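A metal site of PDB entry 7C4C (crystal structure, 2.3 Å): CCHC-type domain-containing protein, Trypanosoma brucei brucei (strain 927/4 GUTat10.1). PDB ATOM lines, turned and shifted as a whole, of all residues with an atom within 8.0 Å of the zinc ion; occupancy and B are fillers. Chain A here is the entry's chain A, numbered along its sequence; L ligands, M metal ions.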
ATOM      1  N   LYS A 280     -13.176  -1.942  -2.942  1.00  0.00           N
ATOM      2  CA  LYS A 280     -12.426  -1.627  -4.162  1.00  0.00           C
ATOM      3  C   LYS A 280     -13.301  -1.869  -5.381  1.00  0.00           C
ATOM      4  O   LYS A 280     -13.928  -2.928  -5.506  1.00  0.00           O
ATOM      5  CB  LYS A 280     -11.151  -2.491  -4.242  1.00  0.00           C
ATOM      6  CG  LYS A 280     -10.094  -2.015  -5.219  1.00  0.00           C
ATOM      7  CD  LYS A 280      -8.856  -2.896  -5.096  1.00  0.00           C
ATOM      8  CE  LYS A 280      -8.513  -3.586  -6.403  1.00  0.00           C
ATOM      9  NZ  LYS A 280      -7.681  -2.711  -7.275  1.00  0.00           N
ATOM     10  N   CYS A 281     -13.307  -0.899  -6.296  1.00  0.00           N
ATOM     11  CA  CYS A 281     -14.246  -0.871  -7.426  1.00  0.00           C
ATOM     12  C   CYS A 281     -13.795  -1.800  -8.552  1.00  0.00           C
ATOM     13  O   CYS A 281     -12.731  -1.592  -9.145  1.00  0.00           O
ATOM     14  CB  CYS A 281     -14.385   0.541  -7.954  1.00  0.00           C
ATOM     15  SG  CYS A 281     -15.527   0.599  -9.306  1.00  0.00           S
ATOM     16  N   SER A 282     -14.624  -2.792  -8.880  1.00  0.00           N
ATOM     17  CA  SER A 282     -14.291  -3.735  -9.948  1.00  0.00           C
ATOM     18  C   SER A 282     -14.322  -3.118 -11.340  1.00  0.00           C
ATOM     19  O   SER A 282     -13.916  -3.788 -12.306  1.00  0.00           O
ATOM     20  CB  SER A 282     -15.253  -4.932  -9.901  1.00  0.00           C
ATOM     21  OG  SER A 282     -16.526  -4.589 -10.414  1.00  0.00           O
ATOM     22  N   PHE A 283     -14.771  -1.872 -11.493  1.00  0.00           N
ATOM     23  CA  PHE A 283     -14.929  -1.252 -12.805  1.00  0.00           C
ATOM     24  C   PHE A 283     -13.902  -0.178 -13.096  1.00  0.00           C
ATOM     25  O   PHE A 283     -13.407  -0.101 -14.222  1.00  0.00           O
ATOM     26  CB  PHE A 283     -16.337  -0.644 -12.938  1.00  0.00           C
ATOM     27  CG  PHE A 283     -16.625  -0.108 -14.323  1.00  0.00           C
ATOM     28  CD1 PHE A 283     -17.051  -0.950 -15.345  1.00  0.00           C
ATOM     29  CD2 PHE A 283     -16.490   1.250 -14.604  1.00  0.00           C
ATOM     30  CE1 PHE A 283     -17.325  -0.459 -16.623  1.00  0.00           C
ATOM     31  CE2 PHE A 283     -16.764   1.748 -15.870  1.00  0.00           C
ATOM     32  CZ  PHE A 283     -17.176   0.890 -16.889  1.00  0.00           C
ATOM     33  N   CYS A 284     -13.568   0.673 -12.133  1.00  0.00           N
ATOM     34  CA  CYS A 284     -12.550   1.699 -12.317  1.00  0.00           C
ATOM     35  C   CYS A 284     -11.291   1.437 -11.493  1.00  0.00           C
ATOM     36  O   CYS A 284     -10.347   2.212 -11.598  1.00  0.00           O
ATOM     37  CB  CYS A 284     -13.110   3.084 -11.987  1.00  0.00           C
ATOM     38  SG  CYS A 284     -13.387   3.344 -10.217  1.00  0.00           S
ATOM     39  N   GLY A 285     -11.269   0.386 -10.678  1.00  0.00           N
ATOM     40  CA  GLY A 285     -10.084   0.041  -9.926  1.00  0.00           C
ATOM     41  C   GLY A 285      -9.864   0.837  -8.647  1.00  0.00           C
ATOM     42  O   GLY A 285      -9.218   0.336  -7.724  1.00  0.00           O
ATOM     43  N   GLU A 286     -10.388   2.065  -8.591  1.00  0.00           N
ATOM     44  CA  GLU A 286     -10.218   2.928  -7.418  1.00  0.00           C
ATOM     45  C   GLU A 286     -10.704   2.218  -6.164  1.00  0.00           C
ATOM     46  O   GLU A 286     -11.672   1.460  -6.176  1.00  0.00           O
ATOM     47  CB  GLU A 286     -10.969   4.246  -7.603  1.00  0.00           C
ATOM     48  CG  GLU A 286     -10.402   5.124  -8.686  1.00  0.00           C
ATOM     49  CD  GLU A 286     -11.265   6.338  -9.031  1.00  0.00           C
ATOM     50  OE1 GLU A 286     -12.107   6.755  -8.183  1.00  0.00           O
ATOM     51  OE2 GLU A 286     -11.117   6.882 -10.153  1.00  0.00           O
ATOM     52  N   VAL A 287     -10.019   2.466  -5.057  1.00  0.00           N
ATOM     53  CA  VAL A 287     -10.381   1.892  -3.776  1.00  0.00           C
ATOM     54  C   VAL A 287     -11.220   2.916  -3.023  1.00  0.00           C
ATOM     55  O   VAL A 287     -10.949   4.122  -3.082  1.00  0.00           O
ATOM     56  CB  VAL A 287      -9.125   1.476  -2.988  1.00  0.00           C
ATOM     57  CG1 VAL A 287      -8.140   2.631  -2.913  1.00  0.00           C
ATOM     58  CG2 VAL A 287      -9.480   0.956  -1.614  1.00  0.00           C
ATOM     59  N   GLY A 288     -12.281   2.444  -2.357  1.00  0.00           N
ATOM     60  CA  GLY A 288     -13.161   3.352  -1.647  1.00  0.00           C
ATOM     61  C   GLY A 288     -14.646   3.201  -1.962  1.00  0.00           C
ATOM     62  O   GLY A 288     -15.475   3.712  -1.198  1.00  0.00           O
ATOM     63  N   HIS A 289     -14.985   2.523  -3.053  1.00  0.00           N
ATOM     64  CA  HIS A 289     -16.376   2.331  -3.437  1.00  0.00           C
ATOM     65  C   HIS A 289     -16.511   1.026  -4.208  1.00  0.00           C
ATOM     66  O   HIS A 289     -15.569   0.574  -4.844  1.00  0.00           O
ATOM     67  CB  HIS A 289     -16.892   3.494  -4.301  1.00  0.00           C
ATOM     68  CG  HIS A 289     -16.150   3.647  -5.594  1.00  0.00           C
ATOM     69  ND1 HIS A 289     -15.016   4.427  -5.707  1.00  0.00           N
ATOM     70  CD2 HIS A 289     -16.374   3.141  -6.832  1.00  0.00           C
ATOM     71  CE1 HIS A 289     -14.580   4.392  -6.961  1.00  0.00           C
ATOM     72  NE2 HIS A 289     -15.379   3.607  -7.661  1.00  0.00           N
ATOM     73  N   THR A 290     -17.688   0.406  -4.121  1.00  0.00           N
ATOM     74  CA  THR A 290     -18.001  -0.751  -4.944  1.00  0.00           C
ATOM     75  C   THR A 290     -18.494  -0.296  -6.312  1.00  0.00           C
ATOM     76  O   THR A 290     -18.725   0.894  -6.551  1.00  0.00           O
ATOM     77  CB  THR A 290     -19.040  -1.623  -4.247  1.00  0.00           C
ATOM     78  OG1 THR A 290     -20.224  -0.858  -3.986  1.00  0.00           O
ATOM     79  CG2 THR A 290     -18.496  -2.138  -2.916  1.00  0.00           C
ATOM     80  N   ALA A 291     -18.671  -1.251  -7.232  1.00  0.00           N
ATOM     81  CA  ALA A 291     -19.093  -0.881  -8.588  1.00  0.00           C
ATOM     82  C   ALA A 291     -20.527  -0.389  -8.626  1.00  0.00           C
ATOM     83  O   ALA A 291     -20.872   0.424  -9.497  1.00  0.00           O
ATOM     84  CB  ALA A 291     -18.924  -2.055  -9.545  1.00  0.00           C
ATOM     85  N   ARG A 292     -21.377  -0.851  -7.702  1.00  0.00           N
ATOM     86  CA  ARG A 292     -22.770  -0.390  -7.663  1.00  0.00           C
ATOM     87  C   ARG A 292     -22.873   1.115  -7.480  1.00  0.00           C
ATOM     88  O   ARG A 292     -23.840   1.727  -7.948  1.00  0.00           O
ATOM     89  CB  ARG A 292     -23.539  -1.110  -6.542  1.00  0.00           C
ATOM     90  N   ASN A 293     -21.863   1.747  -6.836  1.00  0.00           N
ATOM     91  CA  ASN A 293     -21.868   3.185  -6.626  1.00  0.00           C
ATOM     92  C   ASN A 293     -20.767   3.911  -7.408  1.00  0.00           C
ATOM     93  O   ASN A 293     -20.409   5.037  -7.060  1.00  0.00           O
ATOM     94  CB  ASN A 293     -21.736   3.518  -5.134  1.00  0.00           C
ATOM     95  CG  ASN A 293     -22.636   2.660  -4.275  1.00  0.00           C
ATOM     96  OD1 ASN A 293     -23.863   2.705  -4.393  1.00  0.00           O
ATOM     97  ND2 ASN A 293     -22.026   1.905  -3.358  1.00  0.00           N
ATOM     98  N   CYS A 294     -20.244   3.319  -8.484  1.00  0.00           N
ATOM     99  CA  CYS A 294     -19.154   3.923  -9.230  1.00  0.00           C
ATOM    100  C   CYS A 294     -19.663   4.978 -10.204  1.00  0.00           C
ATOM    101  O   CYS A 294     -20.652   4.766 -10.911  1.00  0.00           O
ATOM    102  CB  CYS A 294     -18.378   2.841  -9.978  1.00  0.00           C
ATOM    103  SG  CYS A 294     -17.086   3.455 -11.092  1.00  0.00           S
ATOM    104  N   PHE A 295     -18.988   6.135 -10.237  1.00  0.00           N
ATOM    105  CA  PHE A 295     -19.419   7.235 -11.102  1.00  0.00           C
ATOM    106  C   PHE A 295     -19.039   6.998 -12.546  1.00  0.00           C
ATOM    107  O   PHE A 295     -19.716   7.516 -13.456  1.00  0.00           O
ATOM    108  CB  PHE A 295     -18.834   8.571 -10.656  1.00  0.00           C
ATOM    109  CG  PHE A 295     -19.115   8.943  -9.217  1.00  0.00           C
ATOM    110  CD1 PHE A 295     -20.394   8.885  -8.704  1.00  0.00           C
ATOM    111  CD2 PHE A 295     -18.086   9.384  -8.409  1.00  0.00           C
ATOM    112  CE1 PHE A 295     -20.644   9.236  -7.390  1.00  0.00           C
ATOM    113  CE2 PHE A 295     -18.324   9.734  -7.101  1.00  0.00           C
ATOM    114  CZ  PHE A 295     -19.606   9.666  -6.592  1.00  0.00           C
ATOM    115  N   LYS A 296     -17.968   6.246 -12.796  1.00  0.00           N
ATOM    116  CA  LYS A 296     -17.608   5.937 -14.177  1.00  0.00           C
ATOM    117  C   LYS A 296     -18.586   4.931 -14.780  1.00  0.00           C
ATOM    118  O   LYS A 296     -19.059   5.122 -15.910  1.00  0.00           O
ATOM    119  CB  LYS A 296     -16.165   5.431 -14.260  1.00  0.00           C
ATOM    120  CG  LYS A 296     -15.125   6.461 -13.781  1.00  0.00           C
ATOM    121  CD  LYS A 296     -13.782   6.302 -14.493  1.00  0.00           C
ATOM    122  CE  LYS A 296     -12.745   7.330 -14.004  1.00  0.00           C
ATOM    123  NZ  LYS A 296     -12.356   7.136 -12.577  1.00  0.00           N
ATOM    124  N   LYS A 297     -18.952   3.892 -14.026  1.00  0.00           N
ATOM    125  CA  LYS A 297     -19.907   2.907 -14.526  1.00  0.00           C
ATOM    126  C   LYS A 297     -21.336   3.431 -14.533  1.00  0.00           C
ATOM    127  O   LYS A 297     -22.116   3.062 -15.408  1.00  0.00           O
ATOM    128  CB  LYS A 297     -19.813   1.625 -13.700  1.00  0.00           C
ATOM    129  CG  LYS A 297     -20.623   0.457 -14.236  1.00  0.00           C
ATOM    130  CD  LYS A 297     -20.271  -0.825 -13.501  1.00  0.00           C
ATOM    131  CE  LYS A 297     -20.445  -2.018 -14.418  1.00  0.00           C
ATOM    132  NZ  LYS A 297     -20.611  -3.293 -13.666  1.00  0.00           N
ATOM    133  N   HIS A 298     -21.693   4.276 -13.573  1.00  0.00           N
ATOM    134  CA  HIS A 298     -23.047   4.836 -13.507  1.00  0.00           C
ATOM    135  C   HIS A 298     -22.930   6.348 -13.428  1.00  0.00           C
ATOM    136  O   HIS A 298     -22.976   6.937 -12.341  1.00  0.00           O
ATOM    137  CB  HIS A 298     -23.816   4.260 -12.320  1.00  0.00           C
ATOM    138  CG  HIS A 298     -23.841   2.769 -12.300  1.00  0.00           C
ATOM    139  ND1 HIS A 298     -23.043   2.021 -11.457  1.00  0.00           N
ATOM    140  CD2 HIS A 298     -24.517   1.877 -13.072  1.00  0.00           C
ATOM    141  CE1 HIS A 298     -23.247   0.740 -11.686  1.00  0.00           C
ATOM    142  NE2 HIS A 298     -24.138   0.628 -12.661  1.00  0.00           N
HETATM  143  C1  LIG L   1     -13.246  11.185  -3.414  1.00  0.00           C
HETATM  144  O1  LIG L   1     -14.397  10.702  -4.116  1.00  0.00           O
HETATM  145  C2  LIG L   1     -12.667  10.007  -2.660  1.00  0.00           C
HETATM  146  O2  LIG L   1     -13.087  10.053  -1.298  1.00  0.00           O
HETATM  147  C3  LIG L   1     -13.307   8.777  -3.249  1.00  0.00           C
HETATM  148  O3  LIG L   1     -13.612   7.844  -2.202  1.00  0.00           O
HETATM  149  C4  LIG L   1     -14.569   9.300  -3.894  1.00  0.00           C
HETATM  150  N1  LIG L   1     -14.784   8.600  -5.194  1.00  0.00           N
HETATM  151  C5  LIG L   1     -13.915   8.541  -6.215  1.00  0.00           C
HETATM  152  N2  LIG L   1     -14.486   7.820  -7.215  1.00  0.00           N
HETATM  153  C6  LIG L   1     -15.710   7.420  -6.800  1.00  0.00           C
HETATM  154  C7  LIG L   1     -16.738   6.669  -7.378  1.00  0.00           C
HETATM  155  O4  LIG L   1     -16.619   6.191  -8.532  1.00  0.00           O
HETATM  156  N3  LIG L   1     -17.862   6.454  -6.680  1.00  0.00           N
HETATM  157  C8  LIG L   1     -18.026   6.939  -5.444  1.00  0.00           C
HETATM  158  N4  LIG L   1     -19.178   6.690  -4.776  1.00  0.00           N
HETATM  159  N5  LIG L   1     -17.053   7.674  -4.859  1.00  0.00           N
HETATM  160  C9  LIG L   1     -15.897   7.932  -5.523  1.00  0.00           C
HETATM  161 ZN    ZN M   1     -15.518   2.801  -9.683  1.00  0.00          ZN
HETATM  162 MN    MN M   2     -13.393   8.053  -9.174  1.00  0.00          MN
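The zinc ion is bound by a ring nitrogen (NE2) of His 289 (2.2 Å), the side-chain sulfur (SG) of Cys 294 (2.2 Å), the side-chain sulfur (SG) of Cys 281 (2.2 Å) and the side-chain sulfur (SG) of Cys 284 (2.3 Å). The zinc ion has four donor atoms within binding distance.
Four residues have an atom within 4 Å of the zinc ion: Cys 281, Cys 284, His 289 and Cys 294.
NE2 of His 289 lies close to O4 of the ligand. The backbone NH (N) of Phe 295 sits at hydrogen-bond distance from an oxygen (O4) of the ligand, 2.9 Å away. O4 of the ligand lies close to SG of Cys 294. The backbone carbonyl oxygen (O) of Asn 293 is in hydrogen-bond range of a nitrogen (N3) of the ligand (2.9 Å).
The side-chain sulfur of Cys 281 sits close to the backbone NH of Phe 283 (3.4 Å). SG of Cys 294 lies close to N of Lys 297 (3.5 Å). N of Cys 281 is in hydrogen-bond range of O of Glu 286, at 2.9 Å. The backbone NH (N) of Lys 296 sits close to the side-chain sulfur (SG) of Cys 294 (3.4 Å). The backbone NH of Glu 286 sits close to the side-chain sulfur of Cys 284, at 3.6 Å.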
